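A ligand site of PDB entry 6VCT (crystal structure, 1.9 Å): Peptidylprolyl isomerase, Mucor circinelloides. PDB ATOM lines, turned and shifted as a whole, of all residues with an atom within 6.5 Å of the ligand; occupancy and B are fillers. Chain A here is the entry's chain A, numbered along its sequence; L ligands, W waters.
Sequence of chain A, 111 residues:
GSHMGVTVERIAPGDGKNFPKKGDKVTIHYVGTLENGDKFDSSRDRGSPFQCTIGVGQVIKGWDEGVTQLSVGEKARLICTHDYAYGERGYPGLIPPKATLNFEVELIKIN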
ATOM      1  N   TYR A  30     -22.045   1.012 -19.037  1.00  0.00           N
ATOM      2  CA  TYR A  30     -21.566   2.304 -19.497  1.00  0.00           C
ATOM      3  C   TYR A  30     -22.186   2.667 -20.832  1.00  0.00           C
ATOM      4  O   TYR A  30     -22.540   1.807 -21.635  1.00  0.00           O
ATOM      5  CB  TYR A  30     -20.028   2.340 -19.623  1.00  0.00           C
ATOM      6  CG  TYR A  30     -19.494   1.518 -20.785  1.00  0.00           C
ATOM      7  CD1 TYR A  30     -19.181   0.181 -20.619  1.00  0.00           C
ATOM      8  CD2 TYR A  30     -19.293   2.089 -22.045  1.00  0.00           C
ATOM      9  CE1 TYR A  30     -18.688  -0.581 -21.683  1.00  0.00           C
ATOM     10  CE2 TYR A  30     -18.805   1.338 -23.116  1.00  0.00           C
ATOM     11  CZ  TYR A  30     -18.495   0.007 -22.927  1.00  0.00           C
ATOM     12  OH  TYR A  30     -18.015  -0.761 -23.966  1.00  0.00           O
ATOM     13  N   GLY A  32     -20.658   5.323 -23.685  1.00  0.00           N
ATOM     14  CA  GLY A  32     -19.536   6.174 -24.017  1.00  0.00           C
ATOM     15  C   GLY A  32     -19.928   7.130 -25.121  1.00  0.00           C
ATOM     16  O   GLY A  32     -20.486   6.728 -26.139  1.00  0.00           O
ATOM     17  N   PHE A  40     -20.388   6.645 -28.933  1.00  0.00           N
ATOM     18  CA  PHE A  40     -19.486   5.773 -29.675  1.00  0.00           C
ATOM     19  C   PHE A  40     -19.552   4.306 -29.267  1.00  0.00           C
ATOM     20  O   PHE A  40     -19.119   3.454 -30.034  1.00  0.00           O
ATOM     21  CB  PHE A  40     -18.028   6.266 -29.600  1.00  0.00           C
ATOM     22  CG  PHE A  40     -17.439   6.298 -28.208  1.00  0.00           C
ATOM     23  CD1 PHE A  40     -16.978   5.132 -27.608  1.00  0.00           C
ATOM     24  CD2 PHE A  40     -17.295   7.496 -27.528  1.00  0.00           C
ATOM     25  CE1 PHE A  40     -16.428   5.171 -26.330  1.00  0.00           C
ATOM     26  CE2 PHE A  40     -16.738   7.537 -26.262  1.00  0.00           C
ATOM     27  CZ  PHE A  40     -16.309   6.369 -25.663  1.00  0.00           C
ATOM     28  N   ASP A  41     -20.095   3.991 -28.085  1.00  0.00           N
ATOM     29  CA  ASP A  41     -20.280   2.605 -27.677  1.00  0.00           C
ATOM     30  C   ASP A  41     -21.169   2.584 -26.439  1.00  0.00           C
ATOM     31  O   ASP A  41     -21.354   3.611 -25.776  1.00  0.00           O
ATOM     32  CB  ASP A  41     -18.946   1.893 -27.381  1.00  0.00           C
ATOM     33  CG  ASP A  41     -19.100   0.369 -27.271  1.00  0.00           C
ATOM     34  OD1 ASP A  41     -19.994  -0.200 -27.929  1.00  0.00           O
ATOM     35  OD2 ASP A  41     -18.324  -0.242 -26.519  1.00  0.00           O
ATOM     36  N   SER A  42     -21.722   1.408 -26.149  1.00  0.00           N
ATOM     37  CA  SER A  42     -22.606   1.240 -24.999  1.00  0.00           C
ATOM     38  C   SER A  42     -22.723  -0.228 -24.615  1.00  0.00           C
ATOM     39  O   SER A  42     -23.119  -1.043 -25.462  1.00  0.00           O
ATOM     40  CB  SER A  42     -23.988   1.783 -25.292  1.00  0.00           C
ATOM     41  OG  SER A  42     -24.892   1.391 -24.274  1.00  0.00           O
ATOM     42  N   ARG A  46     -25.904  -3.689 -25.504  1.00  0.00           N
ATOM     43  CA  ARG A  46     -25.601  -5.101 -25.665  1.00  0.00           C
ATOM     44  C   ARG A  46     -26.350  -5.984 -24.666  1.00  0.00           C
ATOM     45  O   ARG A  46     -26.211  -7.215 -24.723  1.00  0.00           O
ATOM     46  CB  ARG A  46     -24.096  -5.338 -25.531  1.00  0.00           C
ATOM     47  CG  ARG A  46     -23.256  -4.441 -26.443  1.00  0.00           C
ATOM     48  CD  ARG A  46     -21.813  -4.913 -26.514  1.00  0.00           C
ATOM     49  NE  ARG A  46     -21.032  -4.562 -25.324  1.00  0.00           N
ATOM     50  CZ  ARG A  46     -20.247  -3.495 -25.219  1.00  0.00           C
ATOM     51  NH1 ARG A  46     -20.168  -2.615 -26.220  1.00  0.00           N
ATOM     52  NH2 ARG A  46     -19.553  -3.291 -24.106  1.00  0.00           N
ATOM     53  N   PHE A  50     -20.338  -4.479 -18.519  1.00  0.00           N
ATOM     54  CA  PHE A  50     -18.920  -4.754 -18.734  1.00  0.00           C
ATOM     55  C   PHE A  50     -18.269  -5.142 -17.414  1.00  0.00           C
ATOM     56  O   PHE A  50     -18.604  -4.597 -16.362  1.00  0.00           O
ATOM     57  CB  PHE A  50     -18.257  -3.510 -19.340  1.00  0.00           C
ATOM     58  CG  PHE A  50     -16.775  -3.596 -19.497  1.00  0.00           C
ATOM     59  CD1 PHE A  50     -16.209  -4.289 -20.566  1.00  0.00           C
ATOM     60  CD2 PHE A  50     -15.937  -2.949 -18.616  1.00  0.00           C
ATOM     61  CE1 PHE A  50     -14.838  -4.344 -20.722  1.00  0.00           C
ATOM     62  CE2 PHE A  50     -14.553  -3.004 -18.766  1.00  0.00           C
ATOM     63  CZ  PHE A  50     -14.004  -3.692 -19.817  1.00  0.00           C
ATOM     64  N   CYS A  52     -14.355  -5.991 -15.538  1.00  0.00           N
ATOM     65  CA  CYS A  52     -12.903  -5.890 -15.667  1.00  0.00           C
ATOM     66  C   CYS A  52     -12.276  -5.887 -14.271  1.00  0.00           C
ATOM     67  O   CYS A  52     -12.977  -5.809 -13.256  1.00  0.00           O
ATOM     68  CB  CYS A  52     -12.475  -4.640 -16.437  1.00  0.00           C
ATOM     69  SG  CYS A  52     -12.753  -3.082 -15.546  1.00  0.00           S
ATOM     70  N   GLN A  58      -5.652  -2.478 -16.893  1.00  0.00           N
ATOM     71  CA  GLN A  58      -6.410  -3.290 -17.837  1.00  0.00           C
ATOM     72  C   GLN A  58      -7.384  -2.468 -18.671  1.00  0.00           C
ATOM     73  O   GLN A  58      -7.772  -2.892 -19.763  1.00  0.00           O
ATOM     74  CB  GLN A  58      -7.180  -4.379 -17.064  1.00  0.00           C
ATOM     75  CG  GLN A  58      -7.802  -5.460 -17.912  1.00  0.00           C
ATOM     76  CD  GLN A  58      -8.423  -6.547 -17.073  1.00  0.00           C
ATOM     77  OE1 GLN A  58      -9.600  -6.471 -16.703  1.00  0.00           O
ATOM     78  NE2 GLN A  58      -7.633  -7.554 -16.726  1.00  0.00           N
ATOM     79  N   VAL A  59      -7.805  -1.302 -18.172  1.00  0.00           N
ATOM     80  CA  VAL A  59      -8.675  -0.401 -18.881  1.00  0.00           C
ATOM     81  C   VAL A  59      -8.008   0.976 -18.924  1.00  0.00           C
ATOM     82  O   VAL A  59      -6.954   1.186 -18.332  1.00  0.00           O
ATOM     83  CB  VAL A  59     -10.085  -0.333 -18.250  1.00  0.00           C
ATOM     84  CG1 VAL A  59     -10.799  -1.663 -18.493  1.00  0.00           C
ATOM     85  CG2 VAL A  59      -9.990  -0.050 -16.755  1.00  0.00           C
ATOM     86  N   ILE A  60      -8.644   1.912 -19.646  1.00  0.00           N
ATOM     87  CA  ILE A  60      -8.068   3.243 -19.761  1.00  0.00           C
ATOM     88  C   ILE A  60      -7.909   3.856 -18.369  1.00  0.00           C
ATOM     89  O   ILE A  60      -8.589   3.486 -17.404  1.00  0.00           O
ATOM     90  CB  ILE A  60      -8.900   4.153 -20.674  1.00  0.00           C
ATOM     91  CG1 ILE A  60     -10.361   4.196 -20.210  1.00  0.00           C
ATOM     92  CG2 ILE A  60      -8.767   3.713 -22.132  1.00  0.00           C
ATOM     93  CD1 ILE A  60     -11.137   5.401 -20.747  1.00  0.00           C
ATOM     94  N   LYS A  61      -6.969   4.796 -18.272  1.00  0.00           N
ATOM     95  CA  LYS A  61      -6.597   5.310 -16.958  1.00  0.00           C
ATOM     96  C   LYS A  61      -7.738   6.095 -16.306  1.00  0.00           C
ATOM     97  O   LYS A  61      -7.828   6.121 -15.073  1.00  0.00           O
ATOM     98  CB  LYS A  61      -5.348   6.172 -17.056  1.00  0.00           C
ATOM     99  CG  LYS A  61      -4.779   6.553 -15.692  1.00  0.00           C
ATOM    100  CD  LYS A  61      -3.796   7.704 -15.783  1.00  0.00           C
ATOM    101  CE  LYS A  61      -2.468   7.349 -15.144  1.00  0.00           C
ATOM    102  NZ  LYS A  61      -1.501   8.474 -15.265  1.00  0.00           N
ATOM    103  N   TRP A  63     -10.802   5.242 -16.257  1.00  0.00           N
ATOM    104  CA  TRP A  63     -11.552   4.241 -15.510  1.00  0.00           C
ATOM    105  C   TRP A  63     -10.799   3.822 -14.251  1.00  0.00           C
ATOM    106  O   TRP A  63     -11.385   3.724 -13.163  1.00  0.00           O
ATOM    107  CB  TRP A  63     -11.843   3.023 -16.387  1.00  0.00           C
ATOM    108  CG  TRP A  63     -13.094   3.155 -17.224  1.00  0.00           C
ATOM    109  CD1 TRP A  63     -13.411   4.184 -18.065  1.00  0.00           C
ATOM    110  CD2 TRP A  63     -14.192   2.243 -17.273  1.00  0.00           C
ATOM    111  NE1 TRP A  63     -14.640   3.965 -18.641  1.00  0.00           N
ATOM    112  CE2 TRP A  63     -15.146   2.783 -18.176  1.00  0.00           C
ATOM    113  CE3 TRP A  63     -14.470   1.023 -16.647  1.00  0.00           C
ATOM    114  CZ2 TRP A  63     -16.343   2.129 -18.472  1.00  0.00           C
ATOM    115  CZ3 TRP A  63     -15.669   0.379 -16.942  1.00  0.00           C
ATOM    116  CH2 TRP A  63     -16.601   0.931 -17.841  1.00  0.00           C
ATOM    117  N   ALA A  85      -7.369   8.640 -21.551  1.00  0.00           N
ATOM    118  CA  ALA A  85      -8.160   7.806 -22.443  1.00  0.00           C
ATOM    119  C   ALA A  85      -7.274   7.284 -23.556  1.00  0.00           C
ATOM    120  O   ALA A  85      -6.348   6.519 -23.296  1.00  0.00           O
ATOM    121  CB  ALA A  85      -9.369   8.582 -22.977  1.00  0.00           C
ATOM    122  N   TYR A  86      -7.495   7.721 -24.806  1.00  0.00           N
ATOM    123  CA  TYR A  86      -6.770   7.157 -25.943  1.00  0.00           C
ATOM    124  C   TYR A  86      -5.690   8.083 -26.496  1.00  0.00           C
ATOM    125  O   TYR A  86      -5.063   7.742 -27.503  1.00  0.00           O
ATOM    126  CB  TYR A  86      -7.771   6.734 -27.023  1.00  0.00           C
ATOM    127  CG  TYR A  86      -8.619   5.602 -26.507  1.00  0.00           C
ATOM    128  CD1 TYR A  86      -8.077   4.335 -26.325  1.00  0.00           C
ATOM    129  CD2 TYR A  86      -9.939   5.814 -26.121  1.00  0.00           C
ATOM    130  CE1 TYR A  86      -8.831   3.293 -25.806  1.00  0.00           C
ATOM    131  CE2 TYR A  86     -10.713   4.769 -25.596  1.00  0.00           C
ATOM    132  CZ  TYR A  86     -10.150   3.519 -25.440  1.00  0.00           C
ATOM    133  OH  TYR A  86     -10.895   2.479 -24.925  1.00  0.00           O
ATOM    134  N   GLY A  87      -5.455   9.226 -25.856  1.00  0.00           N
ATOM    135  CA  GLY A  87      -4.249   9.987 -26.103  1.00  0.00           C
ATOM    136  C   GLY A  87      -4.101  10.491 -27.525  1.00  0.00           C
ATOM    137  O   GLY A  87      -5.081  10.799 -28.228  1.00  0.00           O
ATOM    138  N   ARG A  89      -2.988   8.907 -30.166  1.00  0.00           N
ATOM    139  CA  ARG A  89      -3.279   7.969 -31.238  1.00  0.00           C
ATOM    140  C   ARG A  89      -4.776   7.821 -31.495  1.00  0.00           C
ATOM    141  O   ARG A  89      -5.159   7.453 -32.612  1.00  0.00           O
ATOM    142  CB  ARG A  89      -2.687   6.601 -30.917  1.00  0.00           C
ATOM    143  CG  ARG A  89      -1.159   6.572 -30.910  1.00  0.00           C
ATOM    144  CD  ARG A  89      -0.642   5.130 -30.787  1.00  0.00           C
ATOM    145  NE  ARG A  89      -0.718   4.612 -29.414  1.00  0.00           N
ATOM    146  CZ  ARG A  89      -0.632   3.320 -29.108  1.00  0.00           C
ATOM    147  NH1 ARG A  89      -0.476   2.415 -30.064  1.00  0.00           N
ATOM    148  NH2 ARG A  89      -0.709   2.942 -27.831  1.00  0.00           N
ATOM    149  N   TYR A  91      -8.485   5.920 -31.180  1.00  0.00           N
ATOM    150  CA  TYR A  91      -8.799   4.517 -31.435  1.00  0.00           C
ATOM    151  C   TYR A  91      -9.269   4.373 -32.874  1.00  0.00           C
ATOM    152  O   TYR A  91     -10.284   4.977 -33.255  1.00  0.00           O
ATOM    153  CB  TYR A  91      -9.853   3.939 -30.477  1.00  0.00           C
ATOM    154  CG  TYR A  91      -9.736   2.411 -30.483  1.00  0.00           C
ATOM    155  CD1 TYR A  91     -10.341   1.654 -31.484  1.00  0.00           C
ATOM    156  CD2 TYR A  91      -8.931   1.752 -29.567  1.00  0.00           C
ATOM    157  CE1 TYR A  91     -10.177   0.262 -31.541  1.00  0.00           C
ATOM    158  CE2 TYR A  91      -8.765   0.368 -29.613  1.00  0.00           C
ATOM    159  CZ  TYR A  91      -9.400  -0.363 -30.599  1.00  0.00           C
ATOM    160  OH  TYR A  91      -9.225  -1.736 -30.646  1.00  0.00           O
ATOM    161  N   LEU A  94     -12.893   4.877 -34.549  1.00  0.00           N
ATOM    162  CA  LEU A  94     -13.851   5.155 -33.478  1.00  0.00           C
ATOM    163  C   LEU A  94     -13.600   6.495 -32.794  1.00  0.00           C
ATOM    164  O   LEU A  94     -14.513   7.304 -32.667  1.00  0.00           O
ATOM    165  CB  LEU A  94     -13.816   4.033 -32.435  1.00  0.00           C
ATOM    166  CG  LEU A  94     -15.115   3.479 -31.858  1.00  0.00           C
ATOM    167  CD1 LEU A  94     -16.144   3.219 -32.948  1.00  0.00           C
ATOM    168  CD2 LEU A  94     -14.835   2.204 -31.083  1.00  0.00           C
ATOM    169  N   ILE A  95     -12.378   6.724 -32.332  1.00  0.00           N
ATOM    170  CA  ILE A  95     -12.044   7.855 -31.461  1.00  0.00           C
ATOM    171  C   ILE A  95     -10.943   8.662 -32.135  1.00  0.00           C
ATOM    172  O   ILE A  95      -9.909   8.091 -32.494  1.00  0.00           O
ATOM    173  CB  ILE A  95     -11.580   7.394 -30.065  1.00  0.00           C
ATOM    174  CG1 ILE A  95     -12.581   6.405 -29.463  1.00  0.00           C
ATOM    175  CG2 ILE A  95     -11.384   8.573 -29.139  1.00  0.00           C
ATOM    176  CD1 ILE A  95     -13.778   7.073 -28.873  1.00  0.00           C
ATOM    177  N   LEU A 101     -13.424  12.274 -23.652  1.00  0.00           N
ATOM    178  CA  LEU A 101     -14.457  11.248 -23.718  1.00  0.00           C
ATOM    179  C   LEU A 101     -15.324  11.291 -22.479  1.00  0.00           C
ATOM    180  O   LEU A 101     -14.852  11.598 -21.380  1.00  0.00           O
ATOM    181  CB  LEU A 101     -13.837   9.842 -23.851  1.00  0.00           C
ATOM    182  CG  LEU A 101     -12.971   9.605 -25.087  1.00  0.00           C
ATOM    183  CD1 LEU A 101     -12.586   8.124 -25.159  1.00  0.00           C
ATOM    184  CD2 LEU A 101     -13.695  10.046 -26.341  1.00  0.00           C
ATOM    185  N   PHE A 103     -17.893   8.820 -20.250  1.00  0.00           N
ATOM    186  CA  PHE A 103     -18.465   7.508 -19.953  1.00  0.00           C
ATOM    187  C   PHE A 103     -19.501   7.704 -18.867  1.00  0.00           C
ATOM    188  O   PHE A 103     -19.160   8.010 -17.712  1.00  0.00           O
ATOM    189  CB  PHE A 103     -17.398   6.518 -19.497  1.00  0.00           C
ATOM    190  CG  PHE A 103     -16.473   6.086 -20.578  1.00  0.00           C
ATOM    191  CD1 PHE A 103     -16.775   4.984 -21.371  1.00  0.00           C
ATOM    192  CD2 PHE A 103     -15.291   6.760 -20.808  1.00  0.00           C
ATOM    193  CE1 PHE A 103     -15.903   4.574 -22.377  1.00  0.00           C
ATOM    194  CE2 PHE A 103     -14.416   6.349 -21.805  1.00  0.00           C
ATOM    195  CZ  PHE A 103     -14.728   5.256 -22.592  1.00  0.00           C
HETATM  196  C1  LIG L   1      -6.102   1.108 -24.117  1.00  0.00           C
HETATM  197  C2  LIG L   1     -14.954  -0.251 -21.133  1.00  0.00           C
HETATM  198  C3  LIG L   1      -6.871   0.041 -24.890  1.00  0.00           C
HETATM  199  C4  LIG L   1      -7.962  -0.520 -23.938  1.00  0.00           C
HETATM  200  C5  LIG L   1     -12.601   1.426 -21.894  1.00  0.00           C
HETATM  201  C6  LIG L   1      -9.328  -0.763 -24.394  1.00  0.00           C
HETATM  202  C7  LIG L   1      -9.798  -0.508 -25.840  1.00  0.00           C
HETATM  203  C8  LIG L   1     -10.402  -1.337 -23.300  1.00  0.00           C
HETATM  204  C9  LIG L   1     -11.351   0.542 -22.160  1.00  0.00           C
HETATM  205  C10 LIG L   1     -13.920   1.925 -24.130  1.00  0.00           C
HETATM  206  C11 LIG L   1     -14.543  -0.174 -22.602  1.00  0.00           C
HETATM  207  N1  LIG L   1     -13.690   1.057 -22.925  1.00  0.00           N
HETATM  208  N2  LIG L   1      -8.226  -6.451 -25.201  1.00  0.00           N
HETATM  209  C12 LIG L   1      -4.815   3.777 -23.804  1.00  0.00           C
HETATM  210  N3  LIG L   1      -7.889  -6.410 -23.827  1.00  0.00           N
HETATM  211  C13 LIG L   1      -4.033   0.519 -25.418  1.00  0.00           C
HETATM  212  C14 LIG L   1     -13.894   0.086 -20.172  1.00  0.00           C
HETATM  213  C15 LIG L   1     -13.061   1.257 -20.453  1.00  0.00           C
HETATM  214  C16 LIG L   1     -10.885  -2.788 -23.770  1.00  0.00           C
HETATM  215  C17 LIG L   1      -9.635  -3.698 -24.179  1.00  0.00           C
HETATM  216  C18 LIG L   1     -10.240  -5.072 -24.692  1.00  0.00           C
HETATM  217  C19 LIG L   1      -4.942   1.636 -24.905  1.00  0.00           C
HETATM  218  C20 LIG L   1      -9.232  -5.873 -25.663  1.00  0.00           C
HETATM  219  C21 LIG L   1      -9.522  -6.008 -27.229  1.00  0.00           C
HETATM  220  C22 LIG L   1     -11.026  -6.004 -27.600  1.00  0.00           C
HETATM  221  C23 LIG L   1     -11.989  -6.797 -27.047  1.00  0.00           C
HETATM  222  C24 LIG L   1     -13.430  -6.612 -27.596  1.00  0.00           C
HETATM  223  C25 LIG L   1     -14.258  -5.699 -26.640  1.00  0.00           C
HETATM  224  C26 LIG L   1     -15.720  -6.189 -26.563  1.00  0.00           C
HETATM  225  C27 LIG L   1     -14.148  -4.221 -27.201  1.00  0.00           C
HETATM  226  C28 LIG L   1     -14.339  -3.058 -26.163  1.00  0.00           C
HETATM  227  C29 LIG L   1     -15.500  -3.487 -24.097  1.00  0.00           C
HETATM  228  C30 LIG L   1     -14.442  -1.643 -26.883  1.00  0.00           C
HETATM  229  C31 LIG L   1     -13.242  -1.289 -27.764  1.00  0.00           C
HETATM  230  C32 LIG L   1     -11.992  -2.348 -29.446  1.00  0.00           C
HETATM  231  C33 LIG L   1     -13.237   0.143 -28.178  1.00  0.00           C
HETATM  232  C34 LIG L   1     -13.492   1.081 -27.054  1.00  0.00           C
HETATM  233  C35 LIG L   1     -13.644   2.538 -27.580  1.00  0.00           C
HETATM  234  C36 LIG L   1     -14.760   0.655 -26.320  1.00  0.00           C
HETATM  235  C37 LIG L   1     -15.077   1.532 -25.119  1.00  0.00           C
HETATM  236  C38 LIG L   1     -11.728  -7.849 -25.934  1.00  0.00           C
HETATM  237  C39 LIG L   1      -8.881  -4.857 -28.076  1.00  0.00           C
HETATM  238  C40 LIG L   1      -7.726  -4.106 -27.377  1.00  0.00           C
HETATM  239  C41 LIG L   1      -7.231  -3.040 -27.993  1.00  0.00           C
HETATM  240  C42 LIG L   1      -6.811  -7.312 -23.458  1.00  0.00           C
HETATM  241  C43 LIG L   1      -6.204  -8.176 -24.577  1.00  0.00           C
HETATM  242  C44 LIG L   1     -11.727  -3.436 -22.650  1.00  0.00           C
HETATM  243  C45 LIG L   1      -5.958  -1.089 -25.331  1.00  0.00           C
HETATM  244  C46 LIG L   1      -4.823  -0.538 -26.151  1.00  0.00           C
HETATM  245  O1  LIG L   1      -3.069   1.042 -26.288  1.00  0.00           O
HETATM  246  O2  LIG L   1     -15.834   0.663 -27.226  1.00  0.00           O
HETATM  247  O3  LIG L   1     -16.193   1.902 -24.878  1.00  0.00           O
HETATM  248  O4  LIG L   1      -6.429  -7.362 -22.348  1.00  0.00           O
HETATM  249  O5  LIG L   1      -4.180   2.510 -24.082  1.00  0.00           O
HETATM  250  O6  LIG L   1     -11.451  -0.402 -23.268  1.00  0.00           O
HETATM  251  O7  LIG L   1     -13.239   2.858 -24.307  1.00  0.00           O
HETATM  252  O8  LIG L   1     -10.364   0.632 -21.508  1.00  0.00           O
HETATM  253  O9  LIG L   1      -8.900  -3.927 -23.016  1.00  0.00           O
HETATM  254  O10 LIG L   1     -15.594  -3.206 -25.488  1.00  0.00           O
HETATM  255  O11 LIG L   1     -13.285  -2.062 -28.942  1.00  0.00           O
HETATM  256  O12 LIG L   1     -14.559  -0.687 -25.783  1.00  0.00           O
HETATM  257  O   HOH W   1      -6.180  -2.863 -22.036  1.00  0.00           O
HETATM  258  O   HOH W   2      -2.482  -0.331 -28.682  1.00  0.00           O
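The side-chain hydroxyl (OH) of Tyr 86 lies within hydrogen-bond range of an oxygen (O7) of the ligand, at 2.5 Å. The side-chain carboxylate of Asp 41 sits at hydrogen-bond distance from an oxygen (O2) of the ligand, 2.7 Å away. N of Ile 60 sits at hydrogen-bond distance from O8 of the ligand (2.8 Å). The side-chain hydroxyl (OH) of Tyr 30 lies close to an oxygen (O3) of the ligand. O1 of the ligand sits at hydrogen-bond distance from NH2 of Arg 89, at 3.4 Å.
The side-chain hydroxyl (OH) of Tyr 30 sits at hydrogen-bond distance from the side-chain carboxylate (OD2) of Asp 41 (2.6 Å). The side-chain carboxylate of Asp 41 lies within salt-bridge range of the guanidinium group of Arg 46, 3.0 Å away. The backbone carbonyl oxygen (O) of Asp 41 lies within hydrogen-bond range of the backbone NH (N) of Gly 32 (2.8 Å). OH of Tyr 30 is in hydrogen-bond range of NH2 of Arg 46 (3.0 Å). N of Phe 40 sits at hydrogen-bond distance from O of Gly 32 (2.8 Å).
Residues that only touch the ligand: Phe 40, Phe 50, Gln 58, Val 59, Trp 63, Ala 85, Tyr 91, Leu 94 and Phe 103. Hydrophobic or aromatic side chains that line the ligand: Tyr 30, Phe 40, Phe 50, Val 59, Ile 60, Trp 63, Tyr 86, Tyr 91, Leu 94 and Phe 103. 14 residues have an atom within 4 Å of the ligand: Tyr 30, Phe 40, Asp 41, Phe 50, Gln 58, Val 59, Ile 60, Trp 63, Ala 85, Tyr 86, Arg 89, Tyr 91, Leu 94 and Phe 103. The nearest printed residue that does not touch the ligand is Arg 46 (4.1 Å).
Water W1 lies within hydrogen-bond range of the backbone carbonyl oxygen (O) of Gln 58 (2.8 Å) and an oxygen (O9) of the ligand (3.1 Å).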
